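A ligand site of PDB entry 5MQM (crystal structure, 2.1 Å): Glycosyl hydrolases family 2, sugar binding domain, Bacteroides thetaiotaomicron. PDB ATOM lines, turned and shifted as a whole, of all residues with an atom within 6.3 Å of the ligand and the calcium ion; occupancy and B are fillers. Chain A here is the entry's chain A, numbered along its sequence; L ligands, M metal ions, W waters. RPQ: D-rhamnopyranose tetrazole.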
ATOM      1  N   PHE A  47      24.426 -33.452  -1.590  1.00  0.00           N
ATOM      2  CA  PHE A  47      23.735 -33.943  -2.777  1.00  0.00           C
ATOM      3  C   PHE A  47      24.789 -34.346  -3.843  1.00  0.00           C
ATOM      4  O   PHE A  47      25.746 -33.612  -4.054  1.00  0.00           O
ATOM      5  CB  PHE A  47      22.830 -32.853  -3.360  1.00  0.00           C
ATOM      6  CG  PHE A  47      21.592 -32.612  -2.561  1.00  0.00           C
ATOM      7  CD1 PHE A  47      20.483 -33.418  -2.741  1.00  0.00           C
ATOM      8  CD2 PHE A  47      21.539 -31.608  -1.617  1.00  0.00           C
ATOM      9  CE1 PHE A  47      19.337 -33.233  -1.987  1.00  0.00           C
ATOM     10  CE2 PHE A  47      20.395 -31.410  -0.866  1.00  0.00           C
ATOM     11  CZ  PHE A  47      19.298 -32.204  -1.052  1.00  0.00           C
ATOM     12  N   TYR A  49      24.847 -35.379  -7.808  1.00  0.00           N
ATOM     13  CA  TYR A  49      24.087 -35.308  -9.067  1.00  0.00           C
ATOM     14  C   TYR A  49      24.860 -35.992 -10.205  1.00  0.00           C
ATOM     15  O   TYR A  49      26.025 -35.667 -10.438  1.00  0.00           O
ATOM     16  CB  TYR A  49      23.748 -33.846  -9.437  1.00  0.00           C
ATOM     17  CG  TYR A  49      22.604 -33.205  -8.663  1.00  0.00           C
ATOM     18  CD1 TYR A  49      21.978 -33.872  -7.578  1.00  0.00           C
ATOM     19  CD2 TYR A  49      22.136 -31.941  -8.994  1.00  0.00           C
ATOM     20  CE1 TYR A  49      20.944 -33.287  -6.862  1.00  0.00           C
ATOM     21  CE2 TYR A  49      21.081 -31.359  -8.278  1.00  0.00           C
ATOM     22  CZ  TYR A  49      20.495 -32.048  -7.223  1.00  0.00           C
ATOM     23  OH  TYR A  49      19.442 -31.509  -6.499  1.00  0.00           O
ATOM     24  N   MET A  78      21.168 -38.587  -6.748  1.00  0.00           N
ATOM     25  CA  MET A  78      20.063 -38.118  -7.584  1.00  0.00           C
ATOM     26  C   MET A  78      20.558 -37.860  -9.006  1.00  0.00           C
ATOM     27  O   MET A  78      21.340 -36.953  -9.232  1.00  0.00           O
ATOM     28  CB  MET A  78      19.479 -36.843  -7.000  1.00  0.00           C
ATOM     29  CG  MET A  78      18.833 -37.092  -5.642  1.00  0.00           C
ATOM     30  SD  MET A  78      18.370 -35.606  -4.753  1.00  0.00           S
ATOM     31  CE  MET A  78      17.333 -34.806  -5.966  1.00  0.00           C
ATOM     32  N   ILE A  80      20.188 -36.458 -12.785  1.00  0.00           N
ATOM     33  CA  ILE A  80      19.509 -35.341 -13.371  1.00  0.00           C
ATOM     34  C   ILE A  80      19.686 -35.428 -14.879  1.00  0.00           C
ATOM     35  O   ILE A  80      20.812 -35.452 -15.383  1.00  0.00           O
ATOM     36  CB  ILE A  80      20.109 -34.021 -12.857  1.00  0.00           C
ATOM     37  CG1 ILE A  80      20.207 -34.002 -11.323  1.00  0.00           C
ATOM     38  CG2 ILE A  80      19.293 -32.852 -13.361  1.00  0.00           C
ATOM     39  CD1 ILE A  80      18.885 -34.078 -10.579  1.00  0.00           C
ATOM     40  N   PHE A 126      15.282 -33.940  -9.840  1.00  0.00           N
ATOM     41  CA  PHE A 126      15.243 -33.373  -8.475  1.00  0.00           C
ATOM     42  C   PHE A 126      13.831 -33.046  -7.951  1.00  0.00           C
ATOM     43  O   PHE A 126      13.697 -32.528  -6.849  1.00  0.00           O
ATOM     44  CB  PHE A 126      16.274 -32.226  -8.282  1.00  0.00           C
ATOM     45  CG  PHE A 126      16.202 -31.105  -9.281  1.00  0.00           C
ATOM     46  CD1 PHE A 126      15.055 -30.345  -9.422  1.00  0.00           C
ATOM     47  CD2 PHE A 126      17.338 -30.739 -10.023  1.00  0.00           C
ATOM     48  CE1 PHE A 126      15.030 -29.271 -10.313  1.00  0.00           C
ATOM     49  CE2 PHE A 126      17.317 -29.689 -10.918  1.00  0.00           C
ATOM     50  CZ  PHE A 126      16.155 -28.949 -11.058  1.00  0.00           C
ATOM     51  N   ALA A 127      12.781 -33.393  -8.712  1.00  0.00           N
ATOM     52  CA  ALA A 127      11.382 -33.182  -8.288  1.00  0.00           C
ATOM     53  C   ALA A 127      10.384 -33.802  -9.279  1.00  0.00           C
ATOM     54  O   ALA A 127      10.605 -33.682 -10.490  1.00  0.00           O
ATOM     55  CB  ALA A 127      11.078 -31.688  -8.151  1.00  0.00           C
ATOM     56  N   TRP A 276       6.355 -18.911  -7.663  1.00  0.00           N
ATOM     57  CA  TRP A 276       7.055 -18.901  -8.966  1.00  0.00           C
ATOM     58  C   TRP A 276       6.356 -19.754  -9.980  1.00  0.00           C
ATOM     59  O   TRP A 276       6.559 -19.557 -11.164  1.00  0.00           O
ATOM     60  CB  TRP A 276       8.511 -19.326  -8.816  1.00  0.00           C
ATOM     61  CG  TRP A 276       8.714 -20.701  -8.305  1.00  0.00           C
ATOM     62  CD1 TRP A 276       8.868 -21.075  -7.007  1.00  0.00           C
ATOM     63  CD2 TRP A 276       8.764 -21.886  -9.091  1.00  0.00           C
ATOM     64  NE1 TRP A 276       9.038 -22.451  -6.936  1.00  0.00           N
ATOM     65  CE2 TRP A 276       8.976 -22.969  -8.200  1.00  0.00           C
ATOM     66  CE3 TRP A 276       8.659 -22.145 -10.470  1.00  0.00           C
ATOM     67  CZ2 TRP A 276       9.089 -24.292  -8.639  1.00  0.00           C
ATOM     68  CZ3 TRP A 276       8.764 -23.453 -10.910  1.00  0.00           C
ATOM     69  CH2 TRP A 276       8.977 -24.515  -9.993  1.00  0.00           C
ATOM     70  N   ASP A 458      12.162 -33.793  -2.276  1.00  0.00           N
ATOM     71  CA  ASP A 458      12.690 -32.435  -2.400  1.00  0.00           C
ATOM     72  C   ASP A 458      11.513 -31.438  -2.408  1.00  0.00           C
ATOM     73  O   ASP A 458      10.392 -31.792  -2.054  1.00  0.00           O
ATOM     74  CB  ASP A 458      13.584 -32.319  -3.653  1.00  0.00           C
ATOM     75  CG  ASP A 458      14.784 -31.386  -3.434  1.00  0.00           C
ATOM     76  OD1 ASP A 458      15.845 -31.827  -2.899  1.00  0.00           O
ATOM     77  OD2 ASP A 458      14.658 -30.186  -3.767  1.00  0.00           O
ATOM     78  N   SER A 459      11.796 -30.184  -2.756  1.00  0.00           N
ATOM     79  CA  SER A 459      10.792 -29.110  -2.814  1.00  0.00           C
ATOM     80  C   SER A 459       9.841 -29.251  -4.012  1.00  0.00           C
ATOM     81  O   SER A 459      10.277 -29.541  -5.126  1.00  0.00           O
ATOM     82  CB  SER A 459      11.478 -27.738  -2.777  1.00  0.00           C
ATOM     83  OG  SER A 459      12.692 -27.744  -3.504  1.00  0.00           O
ATOM     84  N   GLU A 461       7.587 -28.938  -7.162  1.00  0.00           N
ATOM     85  CA  GLU A 461       7.640 -28.192  -8.428  1.00  0.00           C
ATOM     86  C   GLU A 461       6.634 -28.710  -9.460  1.00  0.00           C
ATOM     87  O   GLU A 461       6.856 -28.524 -10.639  1.00  0.00           O
ATOM     88  CB  GLU A 461       9.039 -28.283  -9.049  1.00  0.00           C
ATOM     89  CG  GLU A 461      10.169 -27.968  -8.102  1.00  0.00           C
ATOM     90  CD  GLU A 461      11.509 -27.735  -8.793  1.00  0.00           C
ATOM     91  OE1 GLU A 461      11.702 -28.141  -9.972  1.00  0.00           O
ATOM     92  OE2 GLU A 461      12.369 -27.123  -8.106  1.00  0.00           O
ATOM     93  N   GLU A 538      11.614 -31.554   2.028  1.00  0.00           N
ATOM     94  CA  GLU A 538      11.687 -30.100   1.842  1.00  0.00           C
ATOM     95  C   GLU A 538      10.261 -29.539   1.694  1.00  0.00           C
ATOM     96  O   GLU A 538       9.306 -30.218   2.036  1.00  0.00           O
ATOM     97  CB  GLU A 538      12.578 -29.765   0.636  1.00  0.00           C
ATOM     98  CG  GLU A 538      14.048 -30.070   0.862  1.00  0.00           C
ATOM     99  CD  GLU A 538      14.961 -29.460  -0.203  1.00  0.00           C
ATOM    100  OE1 GLU A 538      14.438 -28.851  -1.157  1.00  0.00           O
ATOM    101  OE2 GLU A 538      16.195 -29.621  -0.088  1.00  0.00           O
ATOM    102  N   GLU A 561      16.196 -24.795   2.759  1.00  0.00           N
ATOM    103  CA  GLU A 561      17.130 -24.508   1.686  1.00  0.00           C
ATOM    104  C   GLU A 561      17.599 -23.047   1.789  1.00  0.00           C
ATOM    105  O   GLU A 561      16.808 -22.141   2.117  1.00  0.00           O
ATOM    106  CB  GLU A 561      16.464 -24.915   0.347  1.00  0.00           C
ATOM    107  CG  GLU A 561      16.506 -23.962  -0.808  1.00  0.00           C
ATOM    108  CD  GLU A 561      15.782 -24.511  -2.041  1.00  0.00           C
ATOM    109  OE1 GLU A 561      14.944 -25.424  -1.910  1.00  0.00           O
ATOM    110  OE2 GLU A 561      16.060 -24.001  -3.160  1.00  0.00           O
ATOM    111  N   TRP A 563      20.293 -20.284  -0.413  1.00  0.00           N
ATOM    112  CA  TRP A 563      21.125 -20.057  -1.588  1.00  0.00           C
ATOM    113  C   TRP A 563      22.271 -19.082  -1.325  1.00  0.00           C
ATOM    114  O   TRP A 563      22.217 -18.222  -0.427  1.00  0.00           O
ATOM    115  CB  TRP A 563      20.269 -19.551  -2.734  1.00  0.00           C
ATOM    116  CG  TRP A 563      19.301 -20.548  -3.290  1.00  0.00           C
ATOM    117  CD1 TRP A 563      18.308 -21.234  -2.614  1.00  0.00           C
ATOM    118  CD2 TRP A 563      19.178 -20.942  -4.659  1.00  0.00           C
ATOM    119  NE1 TRP A 563      17.630 -22.040  -3.456  1.00  0.00           N
ATOM    120  CE2 TRP A 563      18.111 -21.868  -4.729  1.00  0.00           C
ATOM    121  CE3 TRP A 563      19.852 -20.584  -5.829  1.00  0.00           C
ATOM    122  CZ2 TRP A 563      17.701 -22.453  -5.932  1.00  0.00           C
ATOM    123  CZ3 TRP A 563      19.451 -21.172  -7.035  1.00  0.00           C
ATOM    124  CH2 TRP A 563      18.381 -22.090  -7.076  1.00  0.00           C
ATOM    125  N   HIS A 569      16.371 -16.399  -6.361  1.00  0.00           N
ATOM    126  CA  HIS A 569      16.017 -17.826  -6.190  1.00  0.00           C
ATOM    127  C   HIS A 569      16.141 -18.362  -4.732  1.00  0.00           C
ATOM    128  O   HIS A 569      15.823 -19.560  -4.452  1.00  0.00           O
ATOM    129  CB  HIS A 569      16.936 -18.677  -7.045  1.00  0.00           C
ATOM    130  CG  HIS A 569      16.600 -18.616  -8.504  1.00  0.00           C
ATOM    131  ND1 HIS A 569      16.734 -17.458  -9.248  1.00  0.00           N
ATOM    132  CD2 HIS A 569      16.141 -19.562  -9.351  1.00  0.00           C
ATOM    133  CE1 HIS A 569      16.341 -17.694 -10.489  1.00  0.00           C
ATOM    134  NE2 HIS A 569      15.983 -18.962 -10.573  1.00  0.00           N
ATOM    135  N   LYS A 571      15.272 -19.029  -0.754  1.00  0.00           N
ATOM    136  CA  LYS A 571      14.014 -19.383  -0.136  1.00  0.00           C
ATOM    137  C   LYS A 571      14.044 -19.282   1.386  1.00  0.00           C
ATOM    138  O   LYS A 571      13.955 -20.282   2.084  1.00  0.00           O
ATOM    139  CB  LYS A 571      13.585 -20.775  -0.617  1.00  0.00           C
ATOM    140  CG  LYS A 571      13.369 -20.827  -2.125  1.00  0.00           C
ATOM    141  CD  LYS A 571      12.656 -22.103  -2.541  1.00  0.00           C
ATOM    142  CE  LYS A 571      12.713 -22.366  -4.032  1.00  0.00           C
ATOM    143  NZ  LYS A 571      13.838 -23.280  -4.409  1.00  0.00           N
ATOM    144  N   ASP A 574      11.100 -20.880   2.945  1.00  0.00           N
ATOM    145  CA  ASP A 574      11.199 -22.361   2.990  1.00  0.00           C
ATOM    146  C   ASP A 574      12.003 -22.788   4.240  1.00  0.00           C
ATOM    147  O   ASP A 574      11.695 -23.804   4.877  1.00  0.00           O
ATOM    148  CB  ASP A 574      11.919 -22.972   1.784  1.00  0.00           C
ATOM    149  CG  ASP A 574      11.072 -23.050   0.521  1.00  0.00           C
ATOM    150  OD1 ASP A 574      10.129 -22.222   0.287  1.00  0.00           O
ATOM    151  OD2 ASP A 574      11.418 -23.978  -0.281  1.00  0.00           O
ATOM    152  N   GLU A 593      19.547 -27.919   2.545  1.00  0.00           N
ATOM    153  CA  GLU A 593      20.254 -27.847   1.257  1.00  0.00           C
ATOM    154  C   GLU A 593      20.918 -26.491   1.214  1.00  0.00           C
ATOM    155  O   GLU A 593      20.232 -25.473   1.174  1.00  0.00           O
ATOM    156  CB  GLU A 593      19.234 -28.014   0.144  1.00  0.00           C
ATOM    157  CG  GLU A 593      19.704 -27.742  -1.266  1.00  0.00           C
ATOM    158  CD  GLU A 593      18.512 -27.471  -2.186  1.00  0.00           C
ATOM    159  OE1 GLU A 593      17.478 -28.194  -2.045  1.00  0.00           O
ATOM    160  OE2 GLU A 593      18.628 -26.532  -3.023  1.00  0.00           O
ATOM    161  N   THR A 596      23.269 -23.425  -2.697  1.00  0.00           N
ATOM    162  CA  THR A 596      22.741 -23.472  -4.065  1.00  0.00           C
ATOM    163  C   THR A 596      22.954 -22.097  -4.687  1.00  0.00           C
ATOM    164  O   THR A 596      22.620 -21.082  -4.092  1.00  0.00           O
ATOM    165  CB  THR A 596      21.261 -23.816  -4.030  1.00  0.00           C
ATOM    166  OG1 THR A 596      21.056 -24.900  -3.124  1.00  0.00           O
ATOM    167  CG2 THR A 596      20.748 -24.180  -5.390  1.00  0.00           C
ATOM    168  N   HIS A 627      24.954 -28.264  -1.536  1.00  0.00           N
ATOM    169  CA  HIS A 627      24.439 -28.259  -2.895  1.00  0.00           C
ATOM    170  C   HIS A 627      25.510 -27.587  -3.756  1.00  0.00           C
ATOM    171  O   HIS A 627      25.682 -26.397  -3.633  1.00  0.00           O
ATOM    172  CB  HIS A 627      23.142 -27.502  -3.000  1.00  0.00           C
ATOM    173  CG  HIS A 627      22.552 -27.584  -4.373  1.00  0.00           C
ATOM    174  ND1 HIS A 627      23.132 -26.983  -5.461  1.00  0.00           N
ATOM    175  CD2 HIS A 627      21.518 -28.317  -4.836  1.00  0.00           C
ATOM    176  CE1 HIS A 627      22.447 -27.286  -6.538  1.00  0.00           C
ATOM    177  NE2 HIS A 627      21.464 -28.092  -6.192  1.00  0.00           N
ATOM    178  N   VAL A 628      26.240 -28.291  -4.616  1.00  0.00           N
ATOM    179  CA  VAL A 628      26.015 -29.665  -5.009  1.00  0.00           C
ATOM    180  C   VAL A 628      27.325 -30.331  -5.421  1.00  0.00           C
ATOM    181  O   VAL A 628      28.228 -29.691  -5.987  1.00  0.00           O
ATOM    182  CB  VAL A 628      24.988 -29.711  -6.175  1.00  0.00           C
ATOM    183  CG1 VAL A 628      25.439 -28.905  -7.380  1.00  0.00           C
ATOM    184  CG2 VAL A 628      24.676 -31.157  -6.558  1.00  0.00           C
ATOM    185  N   LEU A 643      26.155 -29.005 -12.942  1.00  0.00           N
ATOM    186  CA  LEU A 643      24.721 -28.826 -13.206  1.00  0.00           C
ATOM    187  C   LEU A 643      24.511 -27.575 -14.072  1.00  0.00           C
ATOM    188  O   LEU A 643      23.896 -26.573 -13.626  1.00  0.00           O
ATOM    189  CB  LEU A 643      23.970 -28.652 -11.850  1.00  0.00           C
ATOM    190  CG  LEU A 643      22.450 -28.557 -11.825  1.00  0.00           C
ATOM    191  CD1 LEU A 643      21.854 -29.808 -12.474  1.00  0.00           C
ATOM    192  CD2 LEU A 643      21.927 -28.375 -10.402  1.00  0.00           C
ATOM    193  N   ILE A 646      25.194 -24.188 -12.343  1.00  0.00           N
ATOM    194  CA  ILE A 646      24.474 -23.925 -11.112  1.00  0.00           C
ATOM    195  C   ILE A 646      25.404 -24.509 -10.024  1.00  0.00           C
ATOM    196  O   ILE A 646      25.731 -25.704 -10.041  1.00  0.00           O
ATOM    197  CB  ILE A 646      23.081 -24.607 -11.101  1.00  0.00           C
ATOM    198  CG1 ILE A 646      22.148 -23.983 -12.152  1.00  0.00           C
ATOM    199  CG2 ILE A 646      22.414 -24.501  -9.726  1.00  0.00           C
ATOM    200  CD1 ILE A 646      20.834 -24.728 -12.368  1.00  0.00           C
ATOM    201  N   GLY A 647      25.827 -23.651  -9.111  1.00  0.00           N
ATOM    202  CA  GLY A 647      26.682 -24.071  -8.005  1.00  0.00           C
ATOM    203  C   GLY A 647      25.892 -24.492  -6.781  1.00  0.00           C
ATOM    204  O   GLY A 647      24.670 -24.687  -6.865  1.00  0.00           O
HETATM  205  O3  RPQ L   1      16.876 -28.689  -4.965  1.00  0.00           O
HETATM  206  C3  RPQ L   1      16.776 -28.553  -6.386  1.00  0.00           C
HETATM  207  C4  RPQ L   1      18.063 -27.880  -6.919  1.00  0.00           C
HETATM  208  O4  RPQ L   1      19.063 -28.900  -7.149  1.00  0.00           O
HETATM  209  C2  RPQ L   1      15.432 -27.887  -6.736  1.00  0.00           C
HETATM  210  O2  RPQ L   1      14.560 -27.778  -5.603  1.00  0.00           O
HETATM  211  C1  RPQ L   1      15.631 -26.525  -7.270  1.00  0.00           C
HETATM  212  N20 RPQ L   1      14.807 -25.454  -7.191  1.00  0.00           N
HETATM  213  N2  RPQ L   1      15.503 -24.451  -7.861  1.00  0.00           N
HETATM  214  N1  RPQ L   1      16.746 -24.855  -8.359  1.00  0.00           N
HETATM  215  N5  RPQ L   1      16.727 -26.198  -7.926  1.00  0.00           N
HETATM  216  C5  RPQ L   1      17.873 -27.064  -8.213  1.00  0.00           C
HETATM  217  C6  RPQ L   1      19.095 -26.241  -8.631  1.00  0.00           C
HETATM  218 CA    CA M   1      15.296 -27.869  -3.196  1.00  0.00          CA
HETATM  219  O   HOH W   1      12.721 -29.646  -6.117  1.00  0.00           O
HETATM  220  O   HOH W   2      11.810 -25.937  -5.669  1.00  0.00           O
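Water W2 bridges the side-chain carboxylate (OE2) of Glu 461 (2.8 Å) and a nitrogen (N20) of the ligand (3.4 Å).
Within 4 Å of the calcium ion: Asp 458, Ser 459, Glu 538, Glu 561 and Glu 593. The nearest printed residue that does not touch the calcium ion is Lys 571 (5.0 Å).
The calcium ion is bound by the side-chain carboxylate (OE1) of Glu 538 (2.4 Å), the side-chain carboxylate (OD2) of Asp 458 (2.5 Å), the side-chain carboxylate (OE1) of Glu 593 (2.5 Å), an oxygen (O3) of the ligand (2.5 Å), an oxygen (O2) of the ligand (2.5 Å), the side-chain hydroxyl (OG) of Ser 459 (2.6 Å) and the side-chain carboxylate (OE1) of Glu 561 (2.8 Å).
The side-chain carboxylate (OE2) of Glu 593 lies within hydrogen-bond range of the side-chain hydroxyl (OG1) of Thr 596. ND1 of His 627 lies within hydrogen-bond range of O of Gly 647 (3.1 Å). The indole nitrogen (NE1) of Trp 563 lies within hydrogen-bond range of the side-chain carboxylate (OE2) of Glu 561, at 2.5 Å. The side-chain amino group (NZ) of Lys 571 lies within salt-bridge range of the side-chain carboxylate (OE2) of Glu 561, 2.6 Å away. The backbone carbonyl oxygen (O) of His 569 sits at hydrogen-bond distance from the indole nitrogen (NE1) of Trp 563 (3.2 Å).
Merely in contact with the ligand: Trp 563, Phe 126, Lys 571, Ile 646 and Leu 643. Hydrophobic or aromatic side chains within 4 Å of the ligand: Tyr 49, Phe 126, Trp 563, His 627, Leu 643 and Ile 646.
NE2 of His 627 is in hydrogen-bond range of O4 of the ligand (2.7 Å). OH of Tyr 49 is in hydrogen-bond range of O4 of the ligand, at 2.7 Å. OE2 of Glu 461 sits close to O2 of the ligand, at 3.4 Å.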
